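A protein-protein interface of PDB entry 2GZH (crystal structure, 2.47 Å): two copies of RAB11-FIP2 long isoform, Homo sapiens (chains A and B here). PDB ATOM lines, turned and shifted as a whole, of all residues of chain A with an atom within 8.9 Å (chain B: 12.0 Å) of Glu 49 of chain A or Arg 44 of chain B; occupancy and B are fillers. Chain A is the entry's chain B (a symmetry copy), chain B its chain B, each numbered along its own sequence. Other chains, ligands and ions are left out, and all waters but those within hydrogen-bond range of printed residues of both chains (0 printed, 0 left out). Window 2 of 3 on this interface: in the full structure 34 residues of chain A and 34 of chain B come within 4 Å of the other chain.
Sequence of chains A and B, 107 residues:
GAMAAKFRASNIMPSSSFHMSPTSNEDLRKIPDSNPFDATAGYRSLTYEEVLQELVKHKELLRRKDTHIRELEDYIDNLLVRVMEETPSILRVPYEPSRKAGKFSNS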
ATOM      1  N   LEU A  46      -6.751   5.906  22.083  1.00  0.00           N
ATOM      2  CA  LEU A  46      -5.780   6.926  22.466  1.00  0.00           C
ATOM      3  C   LEU A  46      -5.140   7.588  21.277  1.00  0.00           C
ATOM      4  O   LEU A  46      -4.987   6.973  20.225  1.00  0.00           O
ATOM      5  N   THR A  47      -4.763   8.852  21.436  1.00  0.00           N
ATOM      6  CA  THR A  47      -4.041   9.554  20.378  1.00  0.00           C
ATOM      7  C   THR A  47      -2.639   8.974  20.207  1.00  0.00           C
ATOM      8  O   THR A  47      -2.124   8.264  21.071  1.00  0.00           O
ATOM      9  CB  THR A  47      -3.981  11.147  20.543  1.00  0.00           C
ATOM     10  OG1 THR A  47      -2.970  11.543  21.488  1.00  0.00           O
ATOM     11  CG2 THR A  47      -5.358  11.751  20.926  1.00  0.00           C
ATOM     12  N   TYR A  48      -2.039   9.266  19.069  1.00  0.00           N
ATOM     13  CA  TYR A  48      -0.652   8.948  18.829  1.00  0.00           C
ATOM     14  C   TYR A  48       0.252   9.487  19.944  1.00  0.00           C
ATOM     15  O   TYR A  48       1.244   8.838  20.301  1.00  0.00           O
ATOM     16  CB  TYR A  48      -0.224   9.555  17.507  1.00  0.00           C
ATOM     17  CG  TYR A  48       1.136   9.123  17.044  1.00  0.00           C
ATOM     18  CD1 TYR A  48       1.323   7.881  16.420  1.00  0.00           C
ATOM     19  CD2 TYR A  48       2.235   9.964  17.189  1.00  0.00           C
ATOM     20  CE1 TYR A  48       2.581   7.490  15.958  1.00  0.00           C
ATOM     21  CE2 TYR A  48       3.489   9.580  16.734  1.00  0.00           C
ATOM     22  CZ  TYR A  48       3.661   8.341  16.128  1.00  0.00           C
ATOM     23  OH  TYR A  48       4.909   7.961  15.682  1.00  0.00           O
ATOM     24  N   GLU A  49      -0.084  10.675  20.466  1.00  0.00           N
ATOM     25  CA  GLU A  49       0.680  11.303  21.541  1.00  0.00           C
ATOM     26  C   GLU A  49       0.610  10.470  22.800  1.00  0.00           C
ATOM     27  O   GLU A  49       1.620  10.232  23.458  1.00  0.00           O
ATOM     28  CB  GLU A  49       0.198  12.743  21.800  1.00  0.00           C
ATOM     29  CG  GLU A  49       0.776  13.721  20.814  1.00  0.00           C
ATOM     30  CD  GLU A  49       2.189  13.308  20.403  1.00  0.00           C
ATOM     31  OE1 GLU A  49       3.161  13.972  20.845  1.00  0.00           O
ATOM     32  OE2 GLU A  49       2.336  12.288  19.670  1.00  0.00           O
ATOM     33  N   GLU A  50      -0.593   9.997  23.084  1.00  0.00           N
ATOM     34  CA  GLU A  50      -0.871   9.239  24.288  1.00  0.00           C
ATOM     35  C   GLU A  50      -0.239   7.859  24.235  1.00  0.00           C
ATOM     36  O   GLU A  50       0.512   7.501  25.138  1.00  0.00           O
ATOM     37  CB  GLU A  50      -2.375   9.169  24.534  1.00  0.00           C
ATOM     38  CG  GLU A  50      -2.984  10.566  24.637  1.00  0.00           C
ATOM     39  CD  GLU A  50      -4.496  10.563  24.695  1.00  0.00           C
ATOM     40  OE1 GLU A  50      -5.035  11.327  25.529  1.00  0.00           O
ATOM     41  OE2 GLU A  50      -5.138   9.794  23.930  1.00  0.00           O
ATOM     42  N   VAL A  51      -0.513   7.118  23.164  1.00  0.00           N
ATOM     43  CA  VAL A  51       0.099   5.808  22.955  1.00  0.00           C
ATOM     44  C   VAL A  51       1.645   5.912  23.035  1.00  0.00           C
ATOM     45  O   VAL A  51       2.328   4.968  23.427  1.00  0.00           O
ATOM     46  CB  VAL A  51      -0.446   5.131  21.656  1.00  0.00           C
ATOM     47  CG1 VAL A  51       0.167   5.738  20.436  1.00  0.00           C
ATOM     48  CG2 VAL A  51      -0.200   3.647  21.664  1.00  0.00           C
ATOM     49  N   LEU A  52       2.160   7.099  22.748  1.00  0.00           N
ATOM     50  CA  LEU A  52       3.582   7.355  22.732  1.00  0.00           C
ATOM     51  C   LEU A  52       4.203   7.645  24.109  1.00  0.00           C
ATOM     52  O   LEU A  52       5.316   7.201  24.384  1.00  0.00           O
ATOM     53  CB  LEU A  52       3.858   8.502  21.767  1.00  0.00           C
ATOM     54  CG  LEU A  52       5.250   8.757  21.207  1.00  0.00           C
ATOM     55  CD1 LEU A  52       5.621   7.749  20.088  1.00  0.00           C
ATOM     56  CD2 LEU A  52       5.312  10.215  20.716  1.00  0.00           C
ATOM     57  N   GLN A  53       3.519   8.383  24.978  1.00  0.00           N
ATOM     58  CA  GLN A  53       4.013   8.501  26.350  1.00  0.00           C
ATOM     59  C   GLN A  53       3.759   7.207  27.167  1.00  0.00           C
ATOM     60  O   GLN A  53       4.498   6.903  28.120  1.00  0.00           O
ATOM     61  CB  GLN A  53       3.467   9.746  27.049  1.00  0.00           C
ATOM     62  CG  GLN A  53       1.984   9.680  27.423  1.00  0.00           C
ATOM     63  CD  GLN A  53       1.333  11.072  27.443  1.00  0.00           C
ATOM     64  OE1 GLN A  53       1.710  11.964  26.657  1.00  0.00           O
ATOM     65  NE2 GLN A  53       0.344  11.260  28.330  1.00  0.00           N
ATOM     66  N   GLU A  54       2.733   6.455  26.760  1.00  0.00           N
ATOM     67  CA  GLU A  54       2.449   5.140  27.289  1.00  0.00           C
ATOM     68  C   GLU A  54       3.611   4.177  27.082  1.00  0.00           C
ATOM     69  O   GLU A  54       3.928   3.341  27.943  1.00  0.00           O
ATOM     70  CB  GLU A  54       1.262   4.578  26.549  1.00  0.00           C
ATOM     71  CG  GLU A  54       0.514   3.524  27.313  1.00  0.00           C
ATOM     72  CD  GLU A  54      -0.213   4.086  28.525  1.00  0.00           C
ATOM     73  OE1 GLU A  54      -0.200   5.327  28.722  1.00  0.00           O
ATOM     74  OE2 GLU A  54      -0.790   3.274  29.280  1.00  0.00           O
ATOM     75  N   LEU A  55       4.224   4.291  25.912  1.00  0.00           N
ATOM     76  CA  LEU A  55       5.343   3.462  25.527  1.00  0.00           C
ATOM     77  C   LEU A  55       6.566   3.791  26.399  1.00  0.00           C
ATOM     78  O   LEU A  55       7.310   2.897  26.815  1.00  0.00           O
ATOM     79  CB  LEU A  55       5.624   3.712  24.057  1.00  0.00           C
ATOM     80  CG  LEU A  55       6.201   2.651  23.118  1.00  0.00           C
ATOM     81  CD1 LEU A  55       7.738   2.802  23.049  1.00  0.00           C
ATOM     82  CD2 LEU A  55       5.731   1.212  23.430  1.00  0.00           C
ATOM     83  N   VAL A  56       6.725   5.075  26.707  1.00  0.00           N
ATOM     84  CA  VAL A  56       7.826   5.566  27.508  1.00  0.00           C
ATOM     85  C   VAL A  56       7.695   5.112  28.960  1.00  0.00           C
ATOM     86  O   VAL A  56       8.694   4.734  29.597  1.00  0.00           O
ATOM     87  CB  VAL A  56       7.966   7.121  27.361  1.00  0.00           C
ATOM     88  CG1 VAL A  56       8.070   7.854  28.704  1.00  0.00           C
ATOM     89  CG2 VAL A  56       9.142   7.440  26.440  1.00  0.00           C
ATOM     90  N   GLY B  42      10.859  10.153  24.274  1.00  0.00           N
ATOM     91  CA  GLY B  42       9.842  10.681  23.384  1.00  0.00           C
ATOM     92  C   GLY B  42      10.327  10.794  21.953  1.00  0.00           C
ATOM     93  O   GLY B  42      11.044  11.721  21.595  1.00  0.00           O
ATOM     94  N   TYR B  43       9.935   9.833  21.131  1.00  0.00           N
ATOM     95  CA  TYR B  43      10.648   9.551  19.858  1.00  0.00           C
ATOM     96  C   TYR B  43       9.861   8.941  18.644  1.00  0.00           C
ATOM     97  O   TYR B  43       9.461   7.765  18.648  1.00  0.00           O
ATOM     98  CB  TYR B  43      11.964   8.794  20.112  1.00  0.00           C
ATOM     99  CG  TYR B  43      12.926   8.995  18.977  1.00  0.00           C
ATOM    100  CD1 TYR B  43      13.251  10.295  18.543  1.00  0.00           C
ATOM    101  CD2 TYR B  43      13.482   7.904  18.301  1.00  0.00           C
ATOM    102  CE1 TYR B  43      14.115  10.503  17.484  1.00  0.00           C
ATOM    103  CE2 TYR B  43      14.358   8.101  17.238  1.00  0.00           C
ATOM    104  CZ  TYR B  43      14.667   9.404  16.836  1.00  0.00           C
ATOM    105  OH  TYR B  43      15.530   9.607  15.789  1.00  0.00           O
ATOM    106  N   ARG B  44       9.753   9.765  17.592  1.00  0.00           N
ATOM    107  CA  ARG B  44       8.754   9.684  16.501  1.00  0.00           C
ATOM    108  C   ARG B  44       8.824   8.455  15.563  1.00  0.00           C
ATOM    109  O   ARG B  44       8.571   7.318  16.001  1.00  0.00           O
ATOM    110  CB  ARG B  44       8.809  11.000  15.695  1.00  0.00           C
ATOM    111  CG  ARG B  44       7.978  12.181  16.270  1.00  0.00           C
ATOM    112  CD  ARG B  44       8.227  12.562  17.761  1.00  0.00           C
ATOM    113  NE  ARG B  44       6.991  13.029  18.414  1.00  0.00           N
ATOM    114  CZ  ARG B  44       6.866  13.360  19.702  1.00  0.00           C
ATOM    115  NH1 ARG B  44       7.900  13.292  20.542  1.00  0.00           N
ATOM    116  NH2 ARG B  44       5.688  13.758  20.160  1.00  0.00           N
ATOM    117  N   SER B  45       9.119   8.702  14.278  1.00  0.00           N
ATOM    118  CA  SER B  45       9.461   7.643  13.307  1.00  0.00           C
ATOM    119  C   SER B  45       8.392   6.613  12.960  1.00  0.00           C
ATOM    120  O   SER B  45       8.060   6.435  11.790  1.00  0.00           O
ATOM    121  N   LEU B  46       7.854   5.923  13.967  1.00  0.00           N
ATOM    122  CA  LEU B  46       6.963   4.794  13.726  1.00  0.00           C
ATOM    123  C   LEU B  46       5.538   5.221  13.505  1.00  0.00           C
ATOM    124  O   LEU B  46       5.099   6.234  14.041  1.00  0.00           O
ATOM    125  N   THR B  47       4.806   4.449  12.709  1.00  0.00           N
ATOM    126  CA  THR B  47       3.385   4.718  12.509  1.00  0.00           C
ATOM    127  C   THR B  47       2.600   4.441  13.790  1.00  0.00           C
ATOM    128  O   THR B  47       3.077   3.775  14.708  1.00  0.00           O
ATOM    129  CB  THR B  47       2.722   3.961  11.262  1.00  0.00           C
ATOM    130  OG1 THR B  47       2.413   2.592  11.578  1.00  0.00           O
ATOM    131  CG2 THR B  47       3.602   4.046   9.987  1.00  0.00           C
ATOM    132  N   TYR B  48       1.399   4.983  13.847  1.00  0.00           N
ATOM    133  CA  TYR B  48       0.466   4.671  14.903  1.00  0.00           C
ATOM    134  C   TYR B  48       0.264   3.159  15.050  1.00  0.00           C
ATOM    135  O   TYR B  48       0.096   2.665  16.172  1.00  0.00           O
ATOM    136  CB  TYR B  48      -0.869   5.322  14.597  1.00  0.00           C
ATOM    137  CG  TYR B  48      -1.862   5.245  15.718  1.00  0.00           C
ATOM    138  CD1 TYR B  48      -1.793   6.131  16.803  1.00  0.00           C
ATOM    139  CD2 TYR B  48      -2.899   4.318  15.686  1.00  0.00           C
ATOM    140  CE1 TYR B  48      -2.735   6.085  17.832  1.00  0.00           C
ATOM    141  CE2 TYR B  48      -3.838   4.265  16.707  1.00  0.00           C
ATOM    142  CZ  TYR B  48      -3.749   5.142  17.781  1.00  0.00           C
ATOM    143  OH  TYR B  48      -4.681   5.082  18.796  1.00  0.00           O
ATOM    144  N   GLU B  49       0.260   2.443  13.917  1.00  0.00           N
ATOM    145  CA  GLU B  49       0.088   0.992  13.906  1.00  0.00           C
ATOM    146  C   GLU B  49       1.247   0.315  14.602  1.00  0.00           C
ATOM    147  O   GLU B  49       1.056  -0.584  15.417  1.00  0.00           O
ATOM    148  CB  GLU B  49      -0.084   0.461  12.471  1.00  0.00           C
ATOM    149  CG  GLU B  49      -1.491   0.633  11.968  1.00  0.00           C
ATOM    150  CD  GLU B  49      -2.499   0.483  13.107  1.00  0.00           C
ATOM    151  OE1 GLU B  49      -3.197  -0.562  13.158  1.00  0.00           O
ATOM    152  OE2 GLU B  49      -2.566   1.393  13.984  1.00  0.00           O
ATOM    153  N   GLU B  50       2.438   0.804  14.297  1.00  0.00           N
ATOM    154  CA  GLU B  50       3.670   0.238  14.808  1.00  0.00           C
ATOM    155  C   GLU B  50       3.835   0.512  16.292  1.00  0.00           C
ATOM    156  O   GLU B  50       4.017  -0.425  17.066  1.00  0.00           O
ATOM    157  CB  GLU B  50       4.860   0.743  13.999  1.00  0.00           C
ATOM    158  CG  GLU B  50       4.702   0.411  12.516  1.00  0.00           C
ATOM    159  CD  GLU B  50       5.758   1.048  11.639  1.00  0.00           C
ATOM    160  OE1 GLU B  50       6.264   0.329  10.745  1.00  0.00           O
ATOM    161  OE2 GLU B  50       6.091   2.245  11.849  1.00  0.00           O
ATOM    162  N   VAL B  51       3.729   1.781  16.681  1.00  0.00           N
ATOM    163  CA  VAL B  51       3.785   2.164  18.089  1.00  0.00           C
ATOM    164  C   VAL B  51       2.741   1.363  18.912  1.00  0.00           C
ATOM    165  O   VAL B  51       2.935   1.091  20.094  1.00  0.00           O
ATOM    166  CB  VAL B  51       3.699   3.716  18.256  1.00  0.00           C
ATOM    167  CG1 VAL B  51       2.300   4.201  18.062  1.00  0.00           C
ATOM    168  CG2 VAL B  51       4.207   4.154  19.602  1.00  0.00           C
ATOM    169  N   LEU B  52       1.691   0.919  18.237  1.00  0.00           N
ATOM    170  CA  LEU B  52       0.606   0.195  18.858  1.00  0.00           C
ATOM    171  C   LEU B  52       0.860  -1.310  19.054  1.00  0.00           C
ATOM    172  O   LEU B  52       0.470  -1.867  20.078  1.00  0.00           O
ATOM    173  CB  LEU B  52      -0.662   0.423  18.043  1.00  0.00           C
ATOM    174  CG  LEU B  52      -2.043   0.154  18.622  1.00  0.00           C
ATOM    175  CD1 LEU B  52      -2.492   1.270  19.600  1.00  0.00           C
ATOM    176  CD2 LEU B  52      -3.029  -0.022  17.453  1.00  0.00           C
ATOM    177  N   GLN B  53       1.496  -1.981  18.100  1.00  0.00           N
ATOM    178  CA  GLN B  53       1.911  -3.360  18.359  1.00  0.00           C
ATOM    179  C   GLN B  53       3.143  -3.422  19.299  1.00  0.00           C
ATOM    180  O   GLN B  53       3.338  -4.415  20.025  1.00  0.00           O
ATOM    181  CB  GLN B  53       2.126  -4.145  17.067  1.00  0.00           C
ATOM    182  CG  GLN B  53       3.375  -3.755  16.272  1.00  0.00           C
ATOM    183  CD  GLN B  53       3.198  -3.998  14.765  1.00  0.00           C
ATOM    184  OE1 GLN B  53       2.083  -3.866  14.223  1.00  0.00           O
ATOM    185  NE2 GLN B  53       4.299  -4.342  14.079  1.00  0.00           N
ATOM    186  N   GLU B  54       3.938  -2.349  19.290  1.00  0.00           N
ATOM    187  CA  GLU B  54       5.031  -2.158  20.216  1.00  0.00           C
ATOM    188  C   GLU B  54       4.560  -2.153  21.664  1.00  0.00           C
ATOM    189  O   GLU B  54       5.226  -2.681  22.569  1.00  0.00           O
ATOM    190  CB  GLU B  54       5.654  -0.812  19.942  1.00  0.00           C
ATOM    191  CG  GLU B  54       7.079  -0.700  20.396  1.00  0.00           C
ATOM    192  CD  GLU B  54       8.025  -1.564  19.576  1.00  0.00           C
ATOM    193  OE1 GLU B  54       7.571  -2.193  18.588  1.00  0.00           O
ATOM    194  OE2 GLU B  54       9.221  -1.612  19.934  1.00  0.00           O
ATOM    195  N   LEU B  55       3.412  -1.524  21.873  1.00  0.00           N
ATOM    196  CA  LEU B  55       2.805  -1.407  23.179  1.00  0.00           C
ATOM    197  C   LEU B  55       2.341  -2.788  23.669  1.00  0.00           C
ATOM    198  O   LEU B  55       2.485  -3.127  24.848  1.00  0.00           O
ATOM    199  CB  LEU B  55       1.645  -0.436  23.069  1.00  0.00           C
ATOM    200  CG  LEU B  55       1.186   0.462  24.219  1.00  0.00           C
ATOM    201  CD1 LEU B  55       0.039  -0.232  24.991  1.00  0.00           C
ATOM    202  CD2 LEU B  55       2.334   0.959  25.126  1.00  0.00           C
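O of Leu 46 of chain A lies close to OH of Tyr 48 of chain B (2.4 Å). The guanidinium group (NH2) of Arg 44 of chain B is in salt-bridge range of the side-chain carboxylate (OE1) of Glu 49 of chain A, 2.6 Å away. The backbone carbonyl oxygen of Leu 46 of chain B lies close to the side-chain hydroxyl of Tyr 48 of chain A (2.4 Å).
The side-chain hydroxyl of Thr 47 of chain B lies close to the backbone NH of Glu 49 of chain B, 3.2 Å away. N of Thr 47 of chain A is in hydrogen-bond range of OE2 of Glu 50 of chain A (2.7 Å). The backbone NH (N) of Thr 47 of chain B lies within hydrogen-bond range of the side-chain carboxylate (OE2) of Glu 50 of chain B, at 2.7 Å. OG1 of Thr 47 of chain A sits close to N of Glu 49 of chain A, 3.2 Å away.
CE1 of Tyr 48 of chain B touches C of Thr 47 of chain A, 3.7 Å away. Tyr 48 of chain A touches Arg 44 of chain B. C of Thr 47 of chain B touches CE1 of Tyr 48 of chain A, at 3.7 Å. N of Tyr 48 of chain A touches CE1 of Tyr 48 of chain B, at 3.5 Å. Tyr 48 of chain A touches Val 51 of chain B (CE1 to CG1, 3.9 Å). CE1 of Tyr 48 of chain B touches CG1 of Val 51 of chain A, 3.9 Å away. CD2 of Leu 52 of chain A touches NH2 of Arg 44 of chain B (3.6 Å). CG of Glu 54 of chain A touches CD2 of Leu 55 of chain B, at 3.8 Å. CG of Glu 54 of chain B touches CD2 of Leu 55 of chain A (3.8 Å). Leu 55 of chain A touches Leu 55 of chain B.
Printed residues of chain B within 4 Å of Leu 46 of chain A: Tyr 48 (2.4 Å). Of chain B, only Tyr 48 comes within 4 Å of Thr 47 of chain A. Of chain B, only Arg 44, Leu 46, Thr 47, Tyr 48 and Val 51 come within 4 Å of Tyr 48 of chain A. Glu 49 of chain A touches just one residue of chain B: Arg 44 (2.6 Å). No residue of chain B comes within 4 Å of Glu 50 of chain A. Val 51 of chain A touches just these residues of chain B: Tyr 48 (3.9 Å), Val 51 (3.5 Å) and Leu 52 (3.9 Å). Of chain B, only Arg 44 and Val 51 come within 4 Å of Leu 52 of chain A. Printed residues of chain B within 4 Å of Leu 55 of chain A: Glu 54 and Leu 55. Of the printed residues of chain B, Val 56 of chain A touches Gly 42 (3.9 Å). Of chain A, only Tyr 48, Glu 49 and Leu 52 come within 4 Å of Arg 44 of chain B. Ser 45 of chain B touches none of the printed residues of chain A. Leu 46 of chain B touches one residue of chain A. Of the printed residues of chain A, Thr 47 of chain B touches Tyr 48 (3.7 Å). Glu 49 of chain B touches none of the printed residues of chain A. Glu 50 of chain B touches none of the printed residues of chain A. Of the printed residues of chain A, Glu 54 of chain B touches Leu 55. The nearest residue of chain A that does not touch Arg 44 of chain B is Gln 53 of chain A (7.5 Å). The nearest printed residue of chain A that does not touch Thr 47 of chain B is Val 51 of chain A (6.7 Å).
Printed residues of chain A that touch a printed residue of chain B: Leu 46, Thr 47, Tyr 48, Glu 49, Val 51, Leu 52, Glu 54, Leu 55 and Val 56. Hydrophobic or aromatic side chains of chain A within 4 Å of the printed part of chain B: Tyr 48, Val 51, Leu 52, Leu 55 and Val 56. Of the 14 printed residues of chain B, 9 touch a printed residue of chain A. Hydrophobic or aromatic side chains of chain B that line the printed part of chain A: Tyr 48, Val 51, Leu 52 and Leu 55. Among the printed residues, 17 pairs touch across the chains.
Leu 46 of chain A touches Tyr 48 of chain B, and with the chains exchanged Tyr 48 of chain A touches Leu 46 of chain B. Tyr 48 of chain A touches Val 51 of chain B, and with the chains exchanged Val 51 of chain A touches Tyr 48 of chain B. Glu 54 of chain A touches Leu 55 of chain B, and with the chains exchanged Leu 55 of chain A touches Glu 54 of chain B. Leu 55 of chain A touches its own counterpart, Leu 55 of chain B.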
